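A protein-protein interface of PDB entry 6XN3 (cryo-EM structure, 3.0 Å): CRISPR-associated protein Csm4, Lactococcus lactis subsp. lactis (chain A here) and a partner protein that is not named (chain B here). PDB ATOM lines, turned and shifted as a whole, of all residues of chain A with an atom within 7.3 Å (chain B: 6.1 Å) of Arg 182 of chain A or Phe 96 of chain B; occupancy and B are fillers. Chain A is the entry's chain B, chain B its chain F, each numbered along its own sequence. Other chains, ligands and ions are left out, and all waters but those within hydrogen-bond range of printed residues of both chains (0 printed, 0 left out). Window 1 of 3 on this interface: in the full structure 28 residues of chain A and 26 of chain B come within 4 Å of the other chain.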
ATOM      1  N   SER A  10     -15.782  37.822   0.048  1.00  0.00           N
ATOM      2  CA  SER A  10     -16.910  37.471  -0.799  1.00  0.00           C
ATOM      3  C   SER A  10     -18.011  36.933   0.095  1.00  0.00           C
ATOM      4  O   SER A  10     -17.767  36.627   1.266  1.00  0.00           O
ATOM      5  CB  SER A  10     -16.449  36.440  -1.841  1.00  0.00           C
ATOM      6  OG  SER A  10     -16.010  35.254  -1.212  1.00  0.00           O
ATOM      7  N   PRO A  11     -19.255  36.867  -0.389  1.00  0.00           N
ATOM      8  CA  PRO A  11     -20.325  36.299   0.439  1.00  0.00           C
ATOM      9  C   PRO A  11     -20.109  34.820   0.698  1.00  0.00           C
ATOM     10  O   PRO A  11     -19.362  34.143   0.002  1.00  0.00           O
ATOM     11  CB  PRO A  11     -21.587  36.534  -0.389  1.00  0.00           C
ATOM     12  CG  PRO A  11     -21.255  37.642  -1.265  1.00  0.00           C
ATOM     13  CD  PRO A  11     -19.812  37.529  -1.581  1.00  0.00           C
ATOM     14  N   HIS A  13     -22.091  30.996   1.955  1.00  0.00           N
ATOM     15  CA  HIS A  13     -23.342  30.255   2.081  1.00  0.00           C
ATOM     16  C   HIS A  13     -23.036  29.057   2.968  1.00  0.00           C
ATOM     17  O   HIS A  13     -22.520  28.041   2.510  1.00  0.00           O
ATOM     18  CB  HIS A  13     -23.901  29.830   0.737  1.00  0.00           C
ATOM     19  CG  HIS A  13     -24.997  28.818   0.840  1.00  0.00           C
ATOM     20  ND1 HIS A  13     -26.287  29.150   1.182  1.00  0.00           N
ATOM     21  CD2 HIS A  13     -24.989  27.478   0.661  1.00  0.00           C
ATOM     22  CE1 HIS A  13     -27.029  28.060   1.204  1.00  0.00           C
ATOM     23  NE2 HIS A  13     -26.266  27.031   0.889  1.00  0.00           N
ATOM     24  N   SER A 176      -9.751  26.865  -2.709  1.00  0.00           N
ATOM     25  CA  SER A 176     -10.863  25.981  -3.037  1.00  0.00           C
ATOM     26  C   SER A 176     -12.167  26.414  -2.399  1.00  0.00           C
ATOM     27  O   SER A 176     -13.235  26.119  -2.940  1.00  0.00           O
ATOM     28  CB  SER A 176     -10.566  24.545  -2.609  1.00  0.00           C
ATOM     29  OG  SER A 176      -9.549  23.977  -3.404  1.00  0.00           O
ATOM     30  N   GLY A 177     -12.109  27.078  -1.256  1.00  0.00           N
ATOM     31  CA  GLY A 177     -13.288  27.696  -0.698  1.00  0.00           C
ATOM     32  C   GLY A 177     -14.043  26.898   0.340  1.00  0.00           C
ATOM     33  O   GLY A 177     -14.621  25.853   0.040  1.00  0.00           O
ATOM     34  N   ILE A 178     -14.039  27.385   1.569  1.00  0.00           N
ATOM     35  CA  ILE A 178     -14.954  26.893   2.585  1.00  0.00           C
ATOM     36  C   ILE A 178     -16.319  27.478   2.253  1.00  0.00           C
ATOM     37  O   ILE A 178     -16.412  28.525   1.607  1.00  0.00           O
ATOM     38  CB  ILE A 178     -14.451  27.288   3.992  1.00  0.00           C
ATOM     39  CG1 ILE A 178     -15.291  26.701   5.120  1.00  0.00           C
ATOM     40  CG2 ILE A 178     -14.444  28.780   4.170  1.00  0.00           C
ATOM     41  CD1 ILE A 178     -15.444  25.232   5.057  1.00  0.00           C
ATOM     42  N   GLY A 179     -17.378  26.786   2.609  1.00  0.00           N
ATOM     43  CA  GLY A 179     -18.706  27.279   2.335  1.00  0.00           C
ATOM     44  C   GLY A 179     -19.501  26.251   1.568  1.00  0.00           C
ATOM     45  O   GLY A 179     -19.009  25.181   1.236  1.00  0.00           O
ATOM     46  N   GLY A 180     -20.748  26.598   1.298  1.00  0.00           N
ATOM     47  CA  GLY A 180     -21.567  25.645   0.599  1.00  0.00           C
ATOM     48  C   GLY A 180     -21.576  25.802  -0.898  1.00  0.00           C
ATOM     49  O   GLY A 180     -21.126  24.896  -1.595  1.00  0.00           O
ATOM     50  N   LYS A 181     -21.996  26.947  -1.416  1.00  0.00           N
ATOM     51  CA  LYS A 181     -22.353  27.034  -2.828  1.00  0.00           C
ATOM     52  C   LYS A 181     -21.080  27.238  -3.632  1.00  0.00           C
ATOM     53  O   LYS A 181     -20.638  28.356  -3.871  1.00  0.00           O
ATOM     54  CB  LYS A 181     -23.376  28.128  -3.084  1.00  0.00           C
ATOM     55  CG  LYS A 181     -23.983  28.026  -4.465  1.00  0.00           C
ATOM     56  CD  LYS A 181     -24.546  26.645  -4.708  1.00  0.00           C
ATOM     57  CE  LYS A 181     -25.216  26.539  -6.049  1.00  0.00           C
ATOM     58  NZ  LYS A 181     -25.462  25.116  -6.379  1.00  0.00           N
ATOM     59  N   ARG A 182     -20.498  26.127  -4.049  1.00  0.00           N
ATOM     60  CA  ARG A 182     -19.269  26.099  -4.814  1.00  0.00           C
ATOM     61  C   ARG A 182     -19.425  25.142  -5.996  1.00  0.00           C
ATOM     62  O   ARG A 182     -20.148  24.153  -5.903  1.00  0.00           O
ATOM     63  CB  ARG A 182     -18.071  25.693  -3.909  1.00  0.00           C
ATOM     64  CG  ARG A 182     -17.733  26.605  -2.730  1.00  0.00           C
ATOM     65  CD  ARG A 182     -17.444  28.072  -3.077  1.00  0.00           C
ATOM     66  NE  ARG A 182     -16.998  28.310  -4.442  1.00  0.00           N
ATOM     67  CZ  ARG A 182     -16.528  29.459  -4.894  1.00  0.00           C
ATOM     68  NH1 ARG A 182     -16.387  30.487  -4.083  1.00  0.00           N
ATOM     69  NH2 ARG A 182     -16.179  29.568  -6.166  1.00  0.00           N
ATOM     70  N   ASN A 183     -18.746  25.411  -7.116  1.00  0.00           N
ATOM     71  CA  ASN A 183     -17.867  26.549  -7.333  1.00  0.00           C
ATOM     72  C   ASN A 183     -18.537  27.693  -8.064  1.00  0.00           C
ATOM     73  O   ASN A 183     -17.987  28.249  -9.001  1.00  0.00           O
ATOM     74  CB  ASN A 183     -16.659  26.055  -8.085  1.00  0.00           C
ATOM     75  CG  ASN A 183     -15.876  25.050  -7.280  1.00  0.00           C
ATOM     76  OD1 ASN A 183     -15.784  23.881  -7.645  1.00  0.00           O
ATOM     77  ND2 ASN A 183     -15.334  25.490  -6.161  1.00  0.00           N
ATOM     78  N   SER A 184     -19.730  28.054  -7.605  1.00  0.00           N
ATOM     79  CA  SER A 184     -20.413  29.281  -8.005  1.00  0.00           C
ATOM     80  C   SER A 184     -20.732  29.889  -6.652  1.00  0.00           C
ATOM     81  O   SER A 184     -21.875  29.829  -6.198  1.00  0.00           O
ATOM     82  CB  SER A 184     -21.677  28.981  -8.783  1.00  0.00           C
ATOM     83  OG  SER A 184     -21.411  28.166  -9.898  1.00  0.00           O
ATOM     84  N   GLY A 185     -19.752  30.529  -6.039  1.00  0.00           N
ATOM     85  CA  GLY A 185     -18.848  31.487  -6.625  1.00  0.00           C
ATOM     86  C   GLY A 185     -18.636  32.358  -5.401  1.00  0.00           C
ATOM     87  O   GLY A 185     -18.092  33.451  -5.453  1.00  0.00           O
ATOM     88  N   TYR A 186     -19.110  31.829  -4.270  1.00  0.00           N
ATOM     89  CA  TYR A 186     -19.231  32.566  -3.026  1.00  0.00           C
ATOM     90  C   TYR A 186     -18.038  32.401  -2.097  1.00  0.00           C
ATOM     91  O   TYR A 186     -17.308  33.361  -1.858  1.00  0.00           O
ATOM     92  CB  TYR A 186     -20.504  32.101  -2.322  1.00  0.00           C
ATOM     93  CG  TYR A 186     -21.737  32.615  -2.978  1.00  0.00           C
ATOM     94  CD1 TYR A 186     -21.708  33.785  -3.711  1.00  0.00           C
ATOM     95  CD2 TYR A 186     -22.917  31.917  -2.906  1.00  0.00           C
ATOM     96  CE1 TYR A 186     -22.821  34.258  -4.323  1.00  0.00           C
ATOM     97  CE2 TYR A 186     -24.041  32.382  -3.523  1.00  0.00           C
ATOM     98  CZ  TYR A 186     -23.984  33.555  -4.227  1.00  0.00           C
ATOM     99  OH  TYR A 186     -25.097  34.031  -4.852  1.00  0.00           O
ATOM    100  N   GLY A 187     -17.815  31.200  -1.580  1.00  0.00           N
ATOM    101  CA  GLY A 187     -16.881  31.038  -0.486  1.00  0.00           C
ATOM    102  C   GLY A 187     -15.427  31.197  -0.867  1.00  0.00           C
ATOM    103  O   GLY A 187     -14.880  30.367  -1.595  1.00  0.00           O
ATOM    104  N   LYS A 188     -14.804  32.283  -0.420  1.00  0.00           N
ATOM    105  CA  LYS A 188     -13.368  32.457  -0.578  1.00  0.00           C
ATOM    106  C   LYS A 188     -12.882  33.308   0.580  1.00  0.00           C
ATOM    107  O   LYS A 188     -13.644  34.109   1.122  1.00  0.00           O
ATOM    108  CB  LYS A 188     -13.009  33.094  -1.930  1.00  0.00           C
ATOM    109  CG  LYS A 188     -12.808  34.597  -1.925  1.00  0.00           C
ATOM    110  CD  LYS A 188     -12.642  35.149  -3.321  1.00  0.00           C
ATOM    111  CE  LYS A 188     -11.298  34.787  -3.898  1.00  0.00           C
ATOM    112  NZ  LYS A 188     -10.185  35.405  -3.147  1.00  0.00           N
ATOM    113  N   GLN A 242     -19.926  14.522  -0.374  1.00  0.00           N
ATOM    114  CA  GLN A 242     -19.340  15.321  -1.444  1.00  0.00           C
ATOM    115  C   GLN A 242     -18.031  14.669  -1.855  1.00  0.00           C
ATOM    116  O   GLN A 242     -16.973  14.973  -1.302  1.00  0.00           O
ATOM    117  CB  GLN A 242     -19.114  16.760  -1.006  1.00  0.00           C
ATOM    118  CG  GLN A 242     -18.597  17.648  -2.113  1.00  0.00           C
ATOM    119  CD  GLN A 242     -18.129  18.979  -1.601  1.00  0.00           C
ATOM    120  OE1 GLN A 242     -18.721  19.540  -0.691  1.00  0.00           O
ATOM    121  NE2 GLN A 242     -17.048  19.484  -2.170  1.00  0.00           N
ATOM    122  N   GLY B  46     -20.459  35.297  -9.851  1.00  0.00           N
ATOM    123  CA  GLY B  46     -19.610  34.317 -10.501  1.00  0.00           C
ATOM    124  C   GLY B  46     -20.401  33.206 -11.148  1.00  0.00           C
ATOM    125  O   GLY B  46     -19.924  32.562 -12.087  1.00  0.00           O
ATOM    126  N   SER B  47     -21.624  32.978 -10.671  1.00  0.00           N
ATOM    127  CA  SER B  47     -22.502  32.015 -11.313  1.00  0.00           C
ATOM    128  C   SER B  47     -22.925  32.490 -12.694  1.00  0.00           C
ATOM    129  O   SER B  47     -23.090  31.678 -13.603  1.00  0.00           O
ATOM    130  CB  SER B  47     -23.720  31.764 -10.440  1.00  0.00           C
ATOM    131  OG  SER B  47     -24.434  32.964 -10.249  1.00  0.00           O
ATOM    132  N   LEU B  49     -21.117  34.531 -14.820  1.00  0.00           N
ATOM    133  CA  LEU B  49     -19.968  34.339 -15.700  1.00  0.00           C
ATOM    134  C   LEU B  49     -19.734  32.864 -15.989  1.00  0.00           C
ATOM    135  O   LEU B  49     -19.470  32.483 -17.137  1.00  0.00           O
ATOM    136  CB  LEU B  49     -18.725  34.960 -15.073  1.00  0.00           C
ATOM    137  CG  LEU B  49     -17.412  34.724 -15.811  1.00  0.00           C
ATOM    138  CD1 LEU B  49     -17.391  35.478 -17.110  1.00  0.00           C
ATOM    139  CD2 LEU B  49     -16.234  35.116 -14.958  1.00  0.00           C
ATOM    140  N   LYS B  50     -19.872  32.019 -14.964  1.00  0.00           N
ATOM    141  CA  LYS B  50     -19.688  30.582 -15.128  1.00  0.00           C
ATOM    142  C   LYS B  50     -20.738  29.984 -16.048  1.00  0.00           C
ATOM    143  O   LYS B  50     -20.416  29.184 -16.932  1.00  0.00           O
ATOM    144  CB  LYS B  50     -19.733  29.904 -13.766  1.00  0.00           C
ATOM    145  CG  LYS B  50     -19.674  28.403 -13.821  1.00  0.00           C
ATOM    146  CD  LYS B  50     -19.482  27.853 -12.442  1.00  0.00           C
ATOM    147  CE  LYS B  50     -19.770  26.386 -12.395  1.00  0.00           C
ATOM    148  NZ  LYS B  50     -20.360  26.008 -11.093  1.00  0.00           N
ATOM    149  N   MET B  53     -20.107  31.181 -19.722  1.00  0.00           N
ATOM    150  CA  MET B  53     -19.001  30.438 -20.322  1.00  0.00           C
ATOM    151  C   MET B  53     -19.375  28.992 -20.602  1.00  0.00           C
ATOM    152  O   MET B  53     -18.990  28.445 -21.642  1.00  0.00           O
ATOM    153  CB  MET B  53     -17.756  30.481 -19.447  1.00  0.00           C
ATOM    154  CG  MET B  53     -17.109  31.819 -19.310  1.00  0.00           C
ATOM    155  SD  MET B  53     -15.735  31.609 -18.183  1.00  0.00           S
ATOM    156  CE  MET B  53     -14.644  30.644 -19.215  1.00  0.00           C
ATOM    157  N   LEU B  80     -14.467  20.790 -16.776  1.00  0.00           N
ATOM    158  CA  LEU B  80     -14.205  22.177 -16.411  1.00  0.00           C
ATOM    159  C   LEU B  80     -15.201  22.684 -15.375  1.00  0.00           C
ATOM    160  O   LEU B  80     -14.807  23.302 -14.384  1.00  0.00           O
ATOM    161  CB  LEU B  80     -14.222  23.087 -17.637  1.00  0.00           C
ATOM    162  CG  LEU B  80     -13.129  22.972 -18.698  1.00  0.00           C
ATOM    163  CD1 LEU B  80     -13.352  24.014 -19.763  1.00  0.00           C
ATOM    164  CD2 LEU B  80     -11.739  23.087 -18.123  1.00  0.00           C
ATOM    165  N   PHE B  81     -16.495  22.438 -15.574  1.00  0.00           N
ATOM    166  CA  PHE B  81     -17.524  23.083 -14.763  1.00  0.00           C
ATOM    167  C   PHE B  81     -18.354  22.108 -13.934  1.00  0.00           C
ATOM    168  O   PHE B  81     -19.464  22.430 -13.516  1.00  0.00           O
ATOM    169  CB  PHE B  81     -18.445  23.925 -15.636  1.00  0.00           C
ATOM    170  CG  PHE B  81     -17.723  24.886 -16.518  1.00  0.00           C
ATOM    171  CD1 PHE B  81     -17.254  26.081 -16.013  1.00  0.00           C
ATOM    172  CD2 PHE B  81     -17.530  24.609 -17.852  1.00  0.00           C
ATOM    173  CE1 PHE B  81     -16.592  26.970 -16.817  1.00  0.00           C
ATOM    174  CE2 PHE B  81     -16.872  25.498 -18.661  1.00  0.00           C
ATOM    175  CZ  PHE B  81     -16.405  26.681 -18.143  1.00  0.00           C
ATOM    176  N   LEU B  94     -12.788  24.249 -12.189  1.00  0.00           N
ATOM    177  CA  LEU B  94     -12.793  25.697 -12.104  1.00  0.00           C
ATOM    178  C   LEU B  94     -13.423  26.140 -10.797  1.00  0.00           C
ATOM    179  O   LEU B  94     -14.249  25.438 -10.217  1.00  0.00           O
ATOM    180  CB  LEU B  94     -13.545  26.331 -13.274  1.00  0.00           C
ATOM    181  CG  LEU B  94     -12.842  26.550 -14.621  1.00  0.00           C
ATOM    182  CD1 LEU B  94     -11.709  27.513 -14.472  1.00  0.00           C
ATOM    183  CD2 LEU B  94     -12.348  25.302 -15.276  1.00  0.00           C
ATOM    184  N   LYS B  95     -13.024  27.322 -10.346  1.00  0.00           N
ATOM    185  CA  LYS B  95     -13.496  27.928  -9.100  1.00  0.00           C
ATOM    186  C   LYS B  95     -13.703  29.407  -9.415  1.00  0.00           C
ATOM    187  O   LYS B  95     -12.746  30.152  -9.643  1.00  0.00           O
ATOM    188  CB  LYS B  95     -12.492  27.700  -7.984  1.00  0.00           C
ATOM    189  CG  LYS B  95     -12.548  28.641  -6.811  1.00  0.00           C
ATOM    190  CD  LYS B  95     -13.305  28.128  -5.644  1.00  0.00           C
ATOM    191  CE  LYS B  95     -13.098  29.086  -4.495  1.00  0.00           C
ATOM    192  NZ  LYS B  95     -13.472  30.466  -4.880  1.00  0.00           N
ATOM    193  N   PHE B  96     -14.959  29.816  -9.489  1.00  0.00           N
ATOM    194  CA  PHE B  96     -15.269  31.185  -9.851  1.00  0.00           C
ATOM    195  C   PHE B  96     -15.472  32.012  -8.591  1.00  0.00           C
ATOM    196  O   PHE B  96     -15.606  31.487  -7.488  1.00  0.00           O
ATOM    197  CB  PHE B  96     -16.517  31.245 -10.726  1.00  0.00           C
ATOM    198  CG  PHE B  96     -16.306  30.768 -12.134  1.00  0.00           C
ATOM    199  CD1 PHE B  96     -16.244  29.419 -12.424  1.00  0.00           C
ATOM    200  CD2 PHE B  96     -16.195  31.671 -13.166  1.00  0.00           C
ATOM    201  CE1 PHE B  96     -16.060  28.983 -13.708  1.00  0.00           C
ATOM    202  CE2 PHE B  96     -16.011  31.239 -14.451  1.00  0.00           C
ATOM    203  CZ  PHE B  96     -15.942  29.891 -14.721  1.00  0.00           C
ATOM    204  N   ASN B  97     -15.483  33.326  -8.754  1.00  0.00           N
ATOM    205  CA  ASN B  97     -15.760  34.206  -7.635  1.00  0.00           C
ATOM    206  C   ASN B  97     -16.673  35.320  -8.100  1.00  0.00           C
ATOM    207  O   ASN B  97     -16.741  35.628  -9.290  1.00  0.00           O
ATOM    208  CB  ASN B  97     -14.490  34.797  -7.031  1.00  0.00           C
ATOM    209  CG  ASN B  97     -13.608  33.750  -6.418  1.00  0.00           C
ATOM    210  OD1 ASN B  97     -14.005  33.063  -5.484  1.00  0.00           O
ATOM    211  ND2 ASN B  97     -12.402  33.613  -6.943  1.00  0.00           N
ATOM    212  N   ASP B  98     -17.389  35.907  -7.150  1.00  0.00           N
ATOM    213  CA  ASP B  98     -18.228  37.049  -7.461  1.00  0.00           C
ATOM    214  C   ASP B  98     -17.343  38.248  -7.745  1.00  0.00           C
ATOM    215  O   ASP B  98     -16.489  38.608  -6.930  1.00  0.00           O
ATOM    216  CB  ASP B  98     -19.182  37.335  -6.312  1.00  0.00           C
ATOM    217  CG  ASP B  98     -20.419  36.480  -6.370  1.00  0.00           C
ATOM    218  OD1 ASP B  98     -20.379  35.438  -7.049  1.00  0.00           O
ATOM    219  OD2 ASP B  98     -21.432  36.844  -5.739  1.00  0.00           O
ATOM    220  N   GLU B 147     -10.938  37.011 -10.353  1.00  0.00           N
ATOM    221  CA  GLU B 147     -10.039  35.911 -10.041  1.00  0.00           C
ATOM    222  C   GLU B 147     -10.802  34.617 -10.260  1.00  0.00           C
ATOM    223  O   GLU B 147     -11.899  34.447  -9.723  1.00  0.00           O
ATOM    224  CB  GLU B 147      -9.539  35.987  -8.596  1.00  0.00           C
ATOM    225  CG  GLU B 147      -8.692  37.202  -8.264  1.00  0.00           C
ATOM    226  CD  GLU B 147      -8.240  37.216  -6.815  1.00  0.00           C
ATOM    227  OE1 GLU B 147      -8.677  36.336  -6.049  1.00  0.00           O
ATOM    228  OE2 GLU B 147      -7.452  38.106  -6.437  1.00  0.00           O
ATOM    229  N   ILE B 148     -10.233  33.718 -11.052  1.00  0.00           N
ATOM    230  CA  ILE B 148     -10.781  32.385 -11.263  1.00  0.00           C
ATOM    231  C   ILE B 148      -9.688  31.400 -10.888  1.00  0.00           C
ATOM    232  O   ILE B 148      -8.541  31.558 -11.317  1.00  0.00           O
ATOM    233  CB  ILE B 148     -11.228  32.173 -12.715  1.00  0.00           C
ATOM    234  CG1 ILE B 148     -12.342  33.135 -13.095  1.00  0.00           C
ATOM    235  CG2 ILE B 148     -11.765  30.804 -12.897  1.00  0.00           C
ATOM    236  CD1 ILE B 148     -12.662  33.099 -14.569  1.00  0.00           C
ATOM    237  N   PHE B 149     -10.024  30.399 -10.084  1.00  0.00           N
ATOM    238  CA  PHE B 149      -9.029  29.455  -9.595  1.00  0.00           C
ATOM    239  C   PHE B 149      -9.194  28.118 -10.300  1.00  0.00           C
ATOM    240  O   PHE B 149     -10.303  27.590 -10.390  1.00  0.00           O
ATOM    241  CB  PHE B 149      -9.138  29.270  -8.085  1.00  0.00           C
ATOM    242  CG  PHE B 149      -9.038  30.543  -7.299  1.00  0.00           C
ATOM    243  CD1 PHE B 149      -8.255  31.592  -7.733  1.00  0.00           C
ATOM    244  CD2 PHE B 149      -9.704  30.674  -6.099  1.00  0.00           C
ATOM    245  CE1 PHE B 149      -8.166  32.750  -7.003  1.00  0.00           C
ATOM    246  CE2 PHE B 149      -9.616  31.829  -5.368  1.00  0.00           C
ATOM    247  CZ  PHE B 149      -8.845  32.865  -5.819  1.00  0.00           C
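The backbone carbonyl oxygen (O) of Glu 147 of chain B sits at hydrogen-bond distance from the side-chain amide nitrogen (ND2) of Asn 97 of chain B (2.9 Å).
NZ of Lys 95 of chain B sits at hydrogen-bond distance from OD1 of Asn 97 of chain B (2.7 Å).
The backbone NH (N) of Lys 188 of chain A is in hydrogen-bond range of the side-chain hydroxyl (OG) of Ser 10 of chain A (3.3 Å).
NH1 of Arg 182 of chain A is in hydrogen-bond range of O of Gly 187 of chain A (2.9 Å).
OD1 of Asp 98 of chain B sits at hydrogen-bond distance from N of Gly 46 of chain B, at 2.8 Å.
The backbone carbonyl oxygen (O) of Phe 149 of chain B sits at hydrogen-bond distance from the backbone NH (N) of Lys 95 of chain B.
Of the 17 printed residues of chain A, 9 touch a printed residue of chain B.
Printed residues of chain A that touch a printed residue of chain B: Ser 176, Gly 177, Arg 182, Asn 183, Ser 184, Gly 185, Tyr 186, Gly 187 and Lys 188.
Of the 15 printed residues of chain B, 9 touch a printed residue of chain A.
Among the printed residues, 20 pairs touch across the chains.
Of chain B, only Lys 95 (3.0 Å), Phe 96 (2.4 Å) and Asn 97 (3.8 Å) come within 4 Å of Arg 182 of chain A.
Phe 96 of chain B touches just these residues of chain A: Arg 182 (2.4 Å), Asn 183 (3.4 Å) and Gly 185 (3.4 Å).
Of the printed residues of chain A, Lys 50 of chain B touches Asn 183 and Ser 184.
Printed residues of chain A within 4 Å of Asn 97 of chain B: Arg 182, Gly 185 and Lys 188.
Printed residues of chain A within 4 Å of Phe 149 of chain B: Lys 188 (3.7 Å).
Gln 242 of chain A touches none of the printed residues of chain B.
Phe 81 of chain B touches none of the printed residues of chain A.
The side-chain amide oxygen (OD1) of Asn 183 of chain A lies close to the backbone carbonyl oxygen (O) of Leu 94 of chain B (3.4 Å).
NZ of Lys 188 of chain A is in salt-bridge range of OE1 of Glu 147 of chain B (3.4 Å).
The side-chain amino group (NZ) of Lys 50 of chain B lies within hydrogen-bond range of the side-chain hydroxyl (OG) of Ser 184 of chain A (2.7 Å).
The guanidinium group (NH1) of Arg 182 of chain A lies close to the side-chain amino group (NZ) of Lys 95 of chain B (3.0 Å).
The backbone carbonyl oxygen (O) of Asn 183 of chain A sits at hydrogen-bond distance from the backbone NH (N) of Phe 96 of chain B, 3.4 Å away.
The backbone carbonyl oxygen of Gly 185 of chain A is in hydrogen-bond range of the backbone NH of Asp 98 of chain B, 3.1 Å away.
The backbone carbonyl oxygen (O) of Phe 96 of chain B sits close to the guanidinium group (NH2) of Arg 182 of chain A.
Among the printed residues, merely in contact across the chains: Tyr 186 of chain A with Asp 98 of chain B (3.3 Å), Gly 185 of chain A with Asn 97 of chain B (3.3 Å), Lys 188 of chain A with Asn 97 of chain B (3.3 Å), Ser 176 of chain A with Lys 95 of chain B (3.4 Å), Gly 185 of chain A with Phe 96 of chain B (3.4 Å), Asn 183 of chain A with Lys 95 of chain B (3.4 Å), Gly 187 of chain A with Lys 95 of chain B (3.6 Å), Lys 188 of chain A with Phe 149 of chain B (3.7 Å), Asn 183 of chain A with Lys 50 of chain B (3.8 Å), Arg 182 of chain A with Asn 97 of chain B (3.8 Å), Ser 184 of chain A with Ser 47 of chain B (3.8 Å), Gly 177 of chain A with Lys 95 of chain B (3.9 Å) and Lys 188 of chain A with Lys 95 of chain B (3.98 Å).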
